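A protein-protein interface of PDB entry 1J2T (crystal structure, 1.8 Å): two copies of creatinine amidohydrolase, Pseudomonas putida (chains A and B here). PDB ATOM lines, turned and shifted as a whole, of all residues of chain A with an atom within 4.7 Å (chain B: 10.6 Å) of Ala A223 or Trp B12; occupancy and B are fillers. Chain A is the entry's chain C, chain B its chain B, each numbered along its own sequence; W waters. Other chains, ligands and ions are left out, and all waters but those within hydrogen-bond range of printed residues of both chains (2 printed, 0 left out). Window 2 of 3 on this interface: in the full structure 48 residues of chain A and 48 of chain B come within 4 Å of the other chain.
O of Gly B8 is in hydrogen-bond range of N of Met A42 (3.1 Å). The backbone NH of Met A42 sits at hydrogen-bond distance from the backbone carbonyl oxygen of Leu B10 (3.1 Å). The indole nitrogen (NE1) of Trp B12 is in hydrogen-bond range of the backbone carbonyl oxygen (O) of Pro A224, 2.9 Å away. The backbone carbonyl oxygen (O) of Phe A84 is in hydrogen-bond range of the guanidinium group (NH1) of Arg B108 (3.0 Å).
The side-chain hydroxyl (OG1) of Thr B11 lies close to the backbone NH (N) of Lys B13, at 3.4 Å. OE2 of Glu B14 lies within hydrogen-bond range of N of Thr B11 (2.9 Å). The side-chain carboxylate of Glu B16 lies within salt-bridge range of the side-chain amino group of Lys B13 (3.9 Å). The guanidinium group (NH2) of Arg B108 lies within hydrogen-bond range of a ring nitrogen (NE2) of His B109. OE1 of Gln A35 is in hydrogen-bond range of N of Gly A37 (3.0 Å). O of Gly A225 lies within hydrogen-bond range of NE2 of Gln A35, 2.8 Å away.
CB of Gln A35 touches CD1 of Trp B12 (3.5 Å). Gly A37 touches Thr B11. CD1 of Trp B12 touches O of Gly A37 (3.3 Å). His A38 touches Thr B11. His A38 touches Lys B13. O of Val B7 touches CE of Met A42 (3.5 Å). Trp B12 touches Met A42 (CA to SD, 3.7 Å). CB of Tyr B15 touches CE of Met A42 (3.7 Å). Phe A84 touches Trp B12. Pro A85 touches Glu B16.
Gly A37 touches two residues of chain B. Printed residues of chain B within 4 Å of His A38: Thr B11 and Lys B13. Of the printed residues of chain B, Pro A85 touches Trp B12 and Glu B16. No residue of chain B comes within 4 Å of Pro A222. Ala A223 touches just one residue of chain B: Trp B12. No residue of chain B comes within 4 Å of Gly A225. Glu B9 touches none of the printed residues of chain A. Trp B12 touches seven residues of chain A. Of the printed residues of chain A, Tyr B15 touches Met A42. Leu B63 touches none of the printed residues of chain A. Of the printed residues of chain A, Arg B108 touches Phe A84 (3.0 Å).
Of the 12 printed residues of chain A, 8 touch a printed residue of chain B. Hydrophobic or aromatic side chains of chain A within 4 Å of the printed part of chain B: His A38, Met A42, Phe A84 and Pro A85.
No position is printed for both chains. Of the 16 pairs that touch across the chains among the printed residues, none has its exchanged pair printed and touching as well.
Water W1 bridges O of His A38 (2.7 Å) and OG1 of Thr B11 (2.8 Å). Water W2 lies within hydrogen-bond range of O of Gly A37, N of His A36 and N of Trp B12.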
ATOM      1  N   GLN A  35      18.535   9.205   9.801  1.00  0.00           N
ATOM      2  CA  GLN A  35      17.491  10.072  10.319  1.00  0.00           C
ATOM      3  C   GLN A  35      17.378   9.890  11.827  1.00  0.00           C
ATOM      4  O   GLN A  35      17.495   8.773  12.346  1.00  0.00           O
ATOM      5  CB  GLN A  35      16.150   9.786   9.637  1.00  0.00           C
ATOM      6  CG  GLN A  35      15.488   8.448  10.005  1.00  0.00           C
ATOM      7  CD  GLN A  35      14.748   8.462  11.341  1.00  0.00           C
ATOM      8  OE1 GLN A  35      14.347   9.521  11.824  1.00  0.00           O
ATOM      9  NE2 GLN A  35      14.542   7.274  11.924  1.00  0.00           N
ATOM     10  N   HIS A  36      17.198  11.005  12.533  1.00  0.00           N
ATOM     11  CA  HIS A  36      16.987  10.979  13.983  1.00  0.00           C
ATOM     12  C   HIS A  36      15.857  11.940  14.366  1.00  0.00           C
ATOM     13  O   HIS A  36      16.006  12.773  15.269  1.00  0.00           O
ATOM     14  CB  HIS A  36      18.241  11.352  14.753  1.00  0.00           C
ATOM     15  CG  HIS A  36      19.189  10.216  14.977  1.00  0.00           C
ATOM     16  ND1 HIS A  36      20.081   9.789  14.015  1.00  0.00           N
ATOM     17  CD2 HIS A  36      19.401   9.433  16.061  1.00  0.00           C
ATOM     18  CE1 HIS A  36      20.794   8.786  14.500  1.00  0.00           C
ATOM     19  NE2 HIS A  36      20.404   8.553  15.742  1.00  0.00           N
ATOM     20  N   GLY A  37      14.734  11.826  13.670  1.00  0.00           N
ATOM     21  CA  GLY A  37      13.557  12.613  13.983  1.00  0.00           C
ATOM     22  C   GLY A  37      13.561  14.027  13.445  1.00  0.00           C
ATOM     23  O   GLY A  37      14.408  14.390  12.636  1.00  0.00           O
ATOM     24  N   HIS A  38      12.599  14.824  13.902  1.00  0.00           N
ATOM     25  CA  HIS A  38      12.427  16.209  13.455  1.00  0.00           C
ATOM     26  C   HIS A  38      13.306  17.193  14.218  1.00  0.00           C
ATOM     27  O   HIS A  38      13.555  18.310  13.748  1.00  0.00           O
ATOM     28  CB  HIS A  38      10.968  16.657  13.658  1.00  0.00           C
ATOM     29  CG  HIS A  38       9.977  15.986  12.759  1.00  0.00           C
ATOM     30  ND1 HIS A  38       8.703  16.475  12.574  1.00  0.00           N
ATOM     31  CD2 HIS A  38      10.057  14.858  12.014  1.00  0.00           C
ATOM     32  CE1 HIS A  38       8.046  15.690  11.734  1.00  0.00           C
ATOM     33  NE2 HIS A  38       8.846  14.697  11.384  1.00  0.00           N
ATOM     34  N   MET A  42      21.486  14.239  11.570  1.00  0.00           N
ATOM     35  CA  MET A  42      21.668  12.855  11.131  1.00  0.00           C
ATOM     36  C   MET A  42      23.012  12.178  11.428  1.00  0.00           C
ATOM     37  O   MET A  42      23.137  10.960  11.250  1.00  0.00           O
ATOM     38  CB  MET A  42      21.360  12.771   9.622  1.00  0.00           C
ATOM     39  CG  MET A  42      19.874  12.950   9.322  1.00  0.00           C
ATOM     40  SD  MET A  42      19.390  12.657   7.630  1.00  0.00           S
ATOM     41  CE  MET A  42      20.157  14.043   6.821  1.00  0.00           C
ATOM     42  N   PHE A  84      13.721   5.738   5.006  1.00  0.00           N
ATOM     43  CA  PHE A  84      13.771   7.182   5.230  1.00  0.00           C
ATOM     44  C   PHE A  84      14.783   7.875   4.343  1.00  0.00           C
ATOM     45  O   PHE A  84      15.816   7.314   4.008  1.00  0.00           O
ATOM     46  CB  PHE A  84      14.138   7.516   6.674  1.00  0.00           C
ATOM     47  CG  PHE A  84      12.970   7.468   7.607  1.00  0.00           C
ATOM     48  CD1 PHE A  84      12.549   6.267   8.134  1.00  0.00           C
ATOM     49  CD2 PHE A  84      12.274   8.623   7.927  1.00  0.00           C
ATOM     50  CE1 PHE A  84      11.456   6.213   8.986  1.00  0.00           C
ATOM     51  CE2 PHE A  84      11.181   8.574   8.776  1.00  0.00           C
ATOM     52  CZ  PHE A  84      10.771   7.372   9.302  1.00  0.00           C
ATOM     53  N   PRO A  85      14.484   9.116   3.980  1.00  0.00           N
ATOM     54  CA  PRO A  85      15.457   9.950   3.280  1.00  0.00           C
ATOM     55  C   PRO A  85      16.590  10.286   4.226  1.00  0.00           C
ATOM     56  O   PRO A  85      16.400  10.229   5.453  1.00  0.00           O
ATOM     57  CB  PRO A  85      14.684  11.241   2.976  1.00  0.00           C
ATOM     58  CG  PRO A  85      13.289  10.997   3.330  1.00  0.00           C
ATOM     59  CD  PRO A  85      13.213   9.815   4.219  1.00  0.00           C
ATOM     60  N   THR A 221       6.478   2.506  11.740  1.00  0.00           N
ATOM     61  CA  THR A 221       7.418   3.412  12.395  1.00  0.00           C
ATOM     62  C   THR A 221       6.694   4.722  12.655  1.00  0.00           C
ATOM     63  O   THR A 221       6.005   5.210  11.762  1.00  0.00           O
ATOM     64  CB  THR A 221       8.647   3.726  11.480  1.00  0.00           C
ATOM     65  OG1 THR A 221       9.386   2.531  11.201  1.00  0.00           O
ATOM     66  CG2 THR A 221       9.655   4.617  12.201  1.00  0.00           C
ATOM     67  N   PRO A 222       6.843   5.312  13.839  1.00  0.00           N
ATOM     68  CA  PRO A 222       6.227   6.616  14.091  1.00  0.00           C
ATOM     69  C   PRO A 222       6.661   7.594  13.007  1.00  0.00           C
ATOM     70  O   PRO A 222       7.827   7.590  12.624  1.00  0.00           O
ATOM     71  CB  PRO A 222       6.767   7.013  15.464  1.00  0.00           C
ATOM     72  CG  PRO A 222       7.101   5.733  16.126  1.00  0.00           C
ATOM     73  CD  PRO A 222       7.566   4.808  15.018  1.00  0.00           C
ATOM     74  N   ALA A 223       5.731   8.409  12.521  1.00  0.00           N
ATOM     75  CA  ALA A 223       5.986   9.306  11.389  1.00  0.00           C
ATOM     76  C   ALA A 223       7.298  10.095  11.461  1.00  0.00           C
ATOM     77  O   ALA A 223       7.987  10.211  10.458  1.00  0.00           O
ATOM     78  CB  ALA A 223       4.798  10.264  11.192  1.00  0.00           C
ATOM     79  N   PRO A 224       7.638  10.655  12.616  1.00  0.00           N
ATOM     80  CA  PRO A 224       8.880  11.429  12.746  1.00  0.00           C
ATOM     81  C   PRO A 224      10.166  10.609  12.615  1.00  0.00           C
ATOM     82  O   PRO A 224      11.214  11.217  12.413  1.00  0.00           O
ATOM     83  CB  PRO A 224       8.803  12.014  14.166  1.00  0.00           C
ATOM     84  CG  PRO A 224       7.453  11.686  14.691  1.00  0.00           C
ATOM     85  CD  PRO A 224       6.874  10.608  13.873  1.00  0.00           C
ATOM     86  N   GLY A 225      10.093   9.285  12.756  1.00  0.00           N
ATOM     87  CA  GLY A 225      11.266   8.420  12.664  1.00  0.00           C
ATOM     88  C   GLY A 225      11.876   8.025  14.000  1.00  0.00           C
ATOM     89  O   GLY A 225      12.754   7.153  14.080  1.00  0.00           O
ATOM     90  N   LYS B   3      22.181  28.436   7.720  1.00  0.00           N
ATOM     91  CA  LYS B   3      22.005  26.965   7.883  1.00  0.00           C
ATOM     92  C   LYS B   3      23.236  26.219   7.365  1.00  0.00           C
ATOM     93  O   LYS B   3      23.834  26.594   6.350  1.00  0.00           O
ATOM     94  CB  LYS B   3      20.748  26.484   7.144  1.00  0.00           C
ATOM     95  CG  LYS B   3      20.091  25.257   7.771  1.00  0.00           C
ATOM     96  CD  LYS B   3      18.762  24.899   7.111  1.00  0.00           C
ATOM     97  CE  LYS B   3      17.575  25.111   8.042  1.00  0.00           C
ATOM     98  NZ  LYS B   3      16.272  25.036   7.297  1.00  0.00           N
ATOM     99  N   PHE B   6      26.282  20.987   5.683  1.00  0.00           N
ATOM    100  CA  PHE B   6      26.607  19.579   5.921  1.00  0.00           C
ATOM    101  C   PHE B   6      25.365  18.716   6.162  1.00  0.00           C
ATOM    102  O   PHE B   6      24.590  18.953   7.086  1.00  0.00           O
ATOM    103  CB  PHE B   6      27.572  19.441   7.101  1.00  0.00           C
ATOM    104  CG  PHE B   6      28.943  19.976   6.824  1.00  0.00           C
ATOM    105  CD1 PHE B   6      29.330  21.213   7.304  1.00  0.00           C
ATOM    106  CD2 PHE B   6      29.845  19.243   6.078  1.00  0.00           C
ATOM    107  CE1 PHE B   6      30.598  21.715   7.026  1.00  0.00           C
ATOM    108  CE2 PHE B   6      31.110  19.733   5.797  1.00  0.00           C
ATOM    109  CZ  PHE B   6      31.491  20.973   6.288  1.00  0.00           C
ATOM    110  N   VAL B   7      25.184  17.717   5.316  1.00  0.00           N
ATOM    111  CA  VAL B   7      24.055  16.805   5.442  1.00  0.00           C
ATOM    112  C   VAL B   7      23.979  16.217   6.850  1.00  0.00           C
ATOM    113  O   VAL B   7      22.899  16.092   7.408  1.00  0.00           O
ATOM    114  CB  VAL B   7      24.124  15.671   4.393  1.00  0.00           C
ATOM    115  CG1 VAL B   7      23.017  14.641   4.620  1.00  0.00           C
ATOM    116  CG2 VAL B   7      24.014  16.251   2.989  1.00  0.00           C
ATOM    117  N   GLY B   8      25.126  15.878   7.428  1.00  0.00           N
ATOM    118  CA  GLY B   8      25.173  15.289   8.756  1.00  0.00           C
ATOM    119  C   GLY B   8      24.561  16.186   9.826  1.00  0.00           C
ATOM    120  O   GLY B   8      24.078  15.689  10.843  1.00  0.00           O
ATOM    121  N   GLU B   9      24.573  17.493   9.577  1.00  0.00           N
ATOM    122  CA  GLU B   9      24.082  18.490  10.537  1.00  0.00           C
ATOM    123  C   GLU B   9      22.641  18.912  10.274  1.00  0.00           C
ATOM    124  O   GLU B   9      22.120  19.794  10.967  1.00  0.00           O
ATOM    125  CB  GLU B   9      25.009  19.720  10.529  1.00  0.00           C
ATOM    126  CG  GLU B   9      26.401  19.389  11.012  1.00  0.00           C
ATOM    127  CD  GLU B   9      27.327  20.585  11.171  1.00  0.00           C
ATOM    128  OE1 GLU B   9      27.084  21.657  10.581  1.00  0.00           O
ATOM    129  OE2 GLU B   9      28.315  20.430  11.906  1.00  0.00           O
ATOM    130  N   LEU B  10      22.005  18.321   9.266  1.00  0.00           N
ATOM    131  CA  LEU B  10      20.597  18.591   8.977  1.00  0.00           C
ATOM    132  C   LEU B  10      19.707  17.497   9.536  1.00  0.00           C
ATOM    133  O   LEU B  10      20.155  16.380   9.732  1.00  0.00           O
ATOM    134  CB  LEU B  10      20.343  18.654   7.471  1.00  0.00           C
ATOM    135  CG  LEU B  10      21.119  19.680   6.645  1.00  0.00           C
ATOM    136  CD1 LEU B  10      20.695  19.579   5.186  1.00  0.00           C
ATOM    137  CD2 LEU B  10      20.929  21.084   7.178  1.00  0.00           C
ATOM    138  N   THR B  11      18.434  17.810   9.751  1.00  0.00           N
ATOM    139  CA  THR B  11      17.462  16.775  10.091  1.00  0.00           C
ATOM    140  C   THR B  11      17.037  16.105   8.800  1.00  0.00           C
ATOM    141  O   THR B  11      17.216  16.656   7.714  1.00  0.00           O
ATOM    142  CB  THR B  11      16.209  17.348  10.760  1.00  0.00           C
ATOM    143  OG1 THR B  11      15.439  18.083   9.797  1.00  0.00           O
ATOM    144  CG2 THR B  11      16.563  18.325  11.856  1.00  0.00           C
ATOM    145  N   TRP B  12      16.440  14.926   8.899  1.00  0.00           N
ATOM    146  CA  TRP B  12      16.004  14.238   7.698  1.00  0.00           C
ATOM    147  C   TRP B  12      14.932  15.030   6.951  1.00  0.00           C
ATOM    148  O   TRP B  12      14.865  14.973   5.730  1.00  0.00           O
ATOM    149  CB  TRP B  12      15.551  12.814   7.984  1.00  0.00           C
ATOM    150  CG  TRP B  12      14.212  12.637   8.615  1.00  0.00           C
ATOM    151  CD1 TRP B  12      13.952  12.477   9.942  1.00  0.00           C
ATOM    152  CD2 TRP B  12      12.955  12.498   7.943  1.00  0.00           C
ATOM    153  NE1 TRP B  12      12.608  12.268  10.141  1.00  0.00           N
ATOM    154  CE2 TRP B  12      11.971  12.280   8.930  1.00  0.00           C
ATOM    155  CE3 TRP B  12      12.555  12.543   6.606  1.00  0.00           C
ATOM    156  CZ2 TRP B  12      10.626  12.115   8.618  1.00  0.00           C
ATOM    157  CZ3 TRP B  12      11.225  12.378   6.302  1.00  0.00           C
ATOM    158  CH2 TRP B  12      10.272  12.168   7.305  1.00  0.00           C
ATOM    159  N   LYS B  13      14.109  15.776   7.681  1.00  0.00           N
ATOM    160  CA  LYS B  13      13.104  16.632   7.042  1.00  0.00           C
ATOM    161  C   LYS B  13      13.742  17.755   6.221  1.00  0.00           C
ATOM    162  O   LYS B  13      13.295  18.046   5.103  1.00  0.00           O
ATOM    163  CB  LYS B  13      12.153  17.228   8.097  1.00  0.00           C
ATOM    164  CG  LYS B  13      11.330  16.182   8.847  1.00  0.00           C
ATOM    165  CD  LYS B  13      10.271  15.569   7.973  1.00  0.00           C
ATOM    166  CE  LYS B  13       9.131  16.543   7.722  1.00  0.00           C
ATOM    167  NZ  LYS B  13       8.028  15.912   6.939  1.00  0.00           N
ATOM    168  N   GLU B  14      14.767  18.390   6.780  1.00  0.00           N
ATOM    169  CA  GLU B  14      15.478  19.478   6.110  1.00  0.00           C
ATOM    170  C   GLU B  14      16.132  18.960   4.834  1.00  0.00           C
ATOM    171  O   GLU B  14      16.023  19.575   3.776  1.00  0.00           O
ATOM    172  CB  GLU B  14      16.526  20.103   7.043  1.00  0.00           C
ATOM    173  CG  GLU B  14      15.920  20.981   8.142  1.00  0.00           C
ATOM    174  CD  GLU B  14      16.839  21.274   9.328  1.00  0.00           C
ATOM    175  OE1 GLU B  14      16.433  22.115  10.172  1.00  0.00           O
ATOM    176  OE2 GLU B  14      17.936  20.680   9.469  1.00  0.00           O
ATOM    177  N   TYR B  15      16.798  17.813   4.946  1.00  0.00           N
ATOM    178  CA  TYR B  15      17.422  17.152   3.795  1.00  0.00           C
ATOM    179  C   TYR B  15      16.374  16.789   2.726  1.00  0.00           C
ATOM    180  O   TYR B  15      16.523  17.139   1.554  1.00  0.00           O
ATOM    181  CB  TYR B  15      18.190  15.909   4.268  1.00  0.00           C
ATOM    182  CG  TYR B  15      18.778  15.077   3.143  1.00  0.00           C
ATOM    183  CD1 TYR B  15      19.998  15.408   2.563  1.00  0.00           C
ATOM    184  CD2 TYR B  15      18.099  13.984   2.647  1.00  0.00           C
ATOM    185  CE1 TYR B  15      20.517  14.661   1.528  1.00  0.00           C
ATOM    186  CE2 TYR B  15      18.612  13.225   1.611  1.00  0.00           C
ATOM    187  CZ  TYR B  15      19.823  13.567   1.059  1.00  0.00           C
ATOM    188  OH  TYR B  15      20.326  12.788   0.039  1.00  0.00           O
ATOM    189  N   GLU B  16      15.305  16.116   3.136  1.00  0.00           N
ATOM    190  CA  GLU B  16      14.215  15.755   2.240  1.00  0.00           C
ATOM    191  C   GLU B  16      13.687  16.969   1.468  1.00  0.00           C
ATOM    192  O   GLU B  16      13.435  16.902   0.266  1.00  0.00           O
ATOM    193  CB  GLU B  16      13.078  15.127   3.039  1.00  0.00           C
ATOM    194  CG  GLU B  16      11.920  14.638   2.189  1.00  0.00           C
ATOM    195  CD  GLU B  16      10.757  14.141   3.015  1.00  0.00           C
ATOM    196  OE1 GLU B  16      10.233  13.061   2.698  1.00  0.00           O
ATOM    197  OE2 GLU B  16      10.355  14.839   3.974  1.00  0.00           O
ATOM    198  N   ALA B  17      13.519  18.084   2.162  1.00  0.00           N
ATOM    199  CA  ALA B  17      13.023  19.299   1.526  1.00  0.00           C
ATOM    200  C   ALA B  17      14.024  19.854   0.513  1.00  0.00           C
ATOM    201  O   ALA B  17      13.638  20.394  -0.531  1.00  0.00           O
ATOM    202  CB  ALA B  17      12.702  20.356   2.578  1.00  0.00           C
ATOM    203  N   ARG B  18      15.307  19.748   0.822  1.00  0.00           N
ATOM    204  CA  ARG B  18      16.326  20.238  -0.099  1.00  0.00           C
ATOM    205  C   ARG B  18      16.350  19.400  -1.364  1.00  0.00           C
ATOM    206  O   ARG B  18      16.496  19.932  -2.467  1.00  0.00           O
ATOM    207  CB  ARG B  18      17.698  20.269   0.561  1.00  0.00           C
ATOM    208  CG  ARG B  18      17.863  21.411   1.565  1.00  0.00           C
ATOM    209  CD  ARG B  18      17.708  22.798   0.961  1.00  0.00           C
ATOM    210  NE  ARG B  18      18.848  23.137   0.111  1.00  0.00           N
ATOM    211  CZ  ARG B  18      20.019  23.556   0.573  1.00  0.00           C
ATOM    212  NH1 ARG B  18      20.210  23.712   1.872  1.00  0.00           N
ATOM    213  NH2 ARG B  18      21.007  23.832  -0.267  1.00  0.00           N
ATOM    214  N   VAL B  19      16.194  18.093  -1.215  1.00  0.00           N
ATOM    215  CA  VAL B  19      16.173  17.212  -2.377  1.00  0.00           C
ATOM    216  C   VAL B  19      14.879  17.391  -3.162  1.00  0.00           C
ATOM    217  O   VAL B  19      14.880  17.324  -4.386  1.00  0.00           O
ATOM    218  CB  VAL B  19      16.345  15.745  -1.978  1.00  0.00           C
ATOM    219  CG1 VAL B  19      16.148  14.819  -3.183  1.00  0.00           C
ATOM    220  CG2 VAL B  19      17.710  15.539  -1.353  1.00  0.00           C
ATOM    221  N   ALA B  20      13.781  17.642  -2.455  1.00  0.00           N
ATOM    222  CA  ALA B  20      12.481  17.826  -3.090  1.00  0.00           C
ATOM    223  C   ALA B  20      12.465  19.065  -3.993  1.00  0.00           C
ATOM    224  O   ALA B  20      11.693  19.132  -4.947  1.00  0.00           O
ATOM    225  CB  ALA B  20      11.390  17.928  -2.033  1.00  0.00           C
ATOM    226  N   LEU B  63      24.994  20.831  -0.745  1.00  0.00           N
ATOM    227  CA  LEU B  63      25.141  20.159   0.552  1.00  0.00           C
ATOM    228  C   LEU B  63      26.302  19.165   0.526  1.00  0.00           C
ATOM    229  O   LEU B  63      26.590  18.558  -0.505  1.00  0.00           O
ATOM    230  CB  LEU B  63      23.863  19.437   0.945  1.00  0.00           C
ATOM    231  CG  LEU B  63      22.611  20.286   1.137  1.00  0.00           C
ATOM    232  CD1 LEU B  63      21.405  19.383   1.283  1.00  0.00           C
ATOM    233  CD2 LEU B  63      22.772  21.175   2.344  1.00  0.00           C
ATOM    234  N   ARG B 108      18.225   6.561  -4.138  1.00  0.00           N
ATOM    235  CA  ARG B 108      17.000   6.161  -3.451  1.00  0.00           C
ATOM    236  C   ARG B 108      16.277   7.373  -2.864  1.00  0.00           C
ATOM    237  O   ARG B 108      15.037   7.439  -2.891  1.00  0.00           O
ATOM    238  CB  ARG B 108      17.311   5.161  -2.341  1.00  0.00           C
ATOM    239  CG  ARG B 108      16.103   4.749  -1.516  1.00  0.00           C
ATOM    240  CD  ARG B 108      16.411   3.697  -0.476  1.00  0.00           C
ATOM    241  NE  ARG B 108      17.391   4.114   0.532  1.00  0.00           N
ATOM    242  CZ  ARG B 108      17.174   5.018   1.486  1.00  0.00           C
ATOM    243  NH1 ARG B 108      16.016   5.660   1.568  1.00  0.00           N
ATOM    244  NH2 ARG B 108      18.130   5.288   2.362  1.00  0.00           N
ATOM    245  N   HIS B 109      17.047   8.305  -2.309  1.00  0.00           N
ATOM    246  CA  HIS B 109      16.502   9.540  -1.727  1.00  0.00           C
ATOM    247  C   HIS B 109      15.838  10.425  -2.766  1.00  0.00           C
ATOM    248  O   HIS B 109      15.053  11.333  -2.423  1.00  0.00           O
ATOM    249  CB  HIS B 109      17.596  10.406  -1.119  1.00  0.00           C
ATOM    250  CG  HIS B 109      18.394   9.756  -0.037  1.00  0.00           C
ATOM    251  ND1 HIS B 109      19.577  10.290   0.415  1.00  0.00           N
ATOM    252  CD2 HIS B 109      18.201   8.613   0.667  1.00  0.00           C
ATOM    253  CE1 HIS B 109      20.070   9.521   1.368  1.00  0.00           C
ATOM    254  NE2 HIS B 109      19.260   8.493   1.534  1.00  0.00           N
HETATM  255  O   HOH W   1      13.187  18.965  11.206  1.00  0.00           O
HETATM  256  O   HOH W   2      16.813  13.742  11.666  1.00  0.00           O
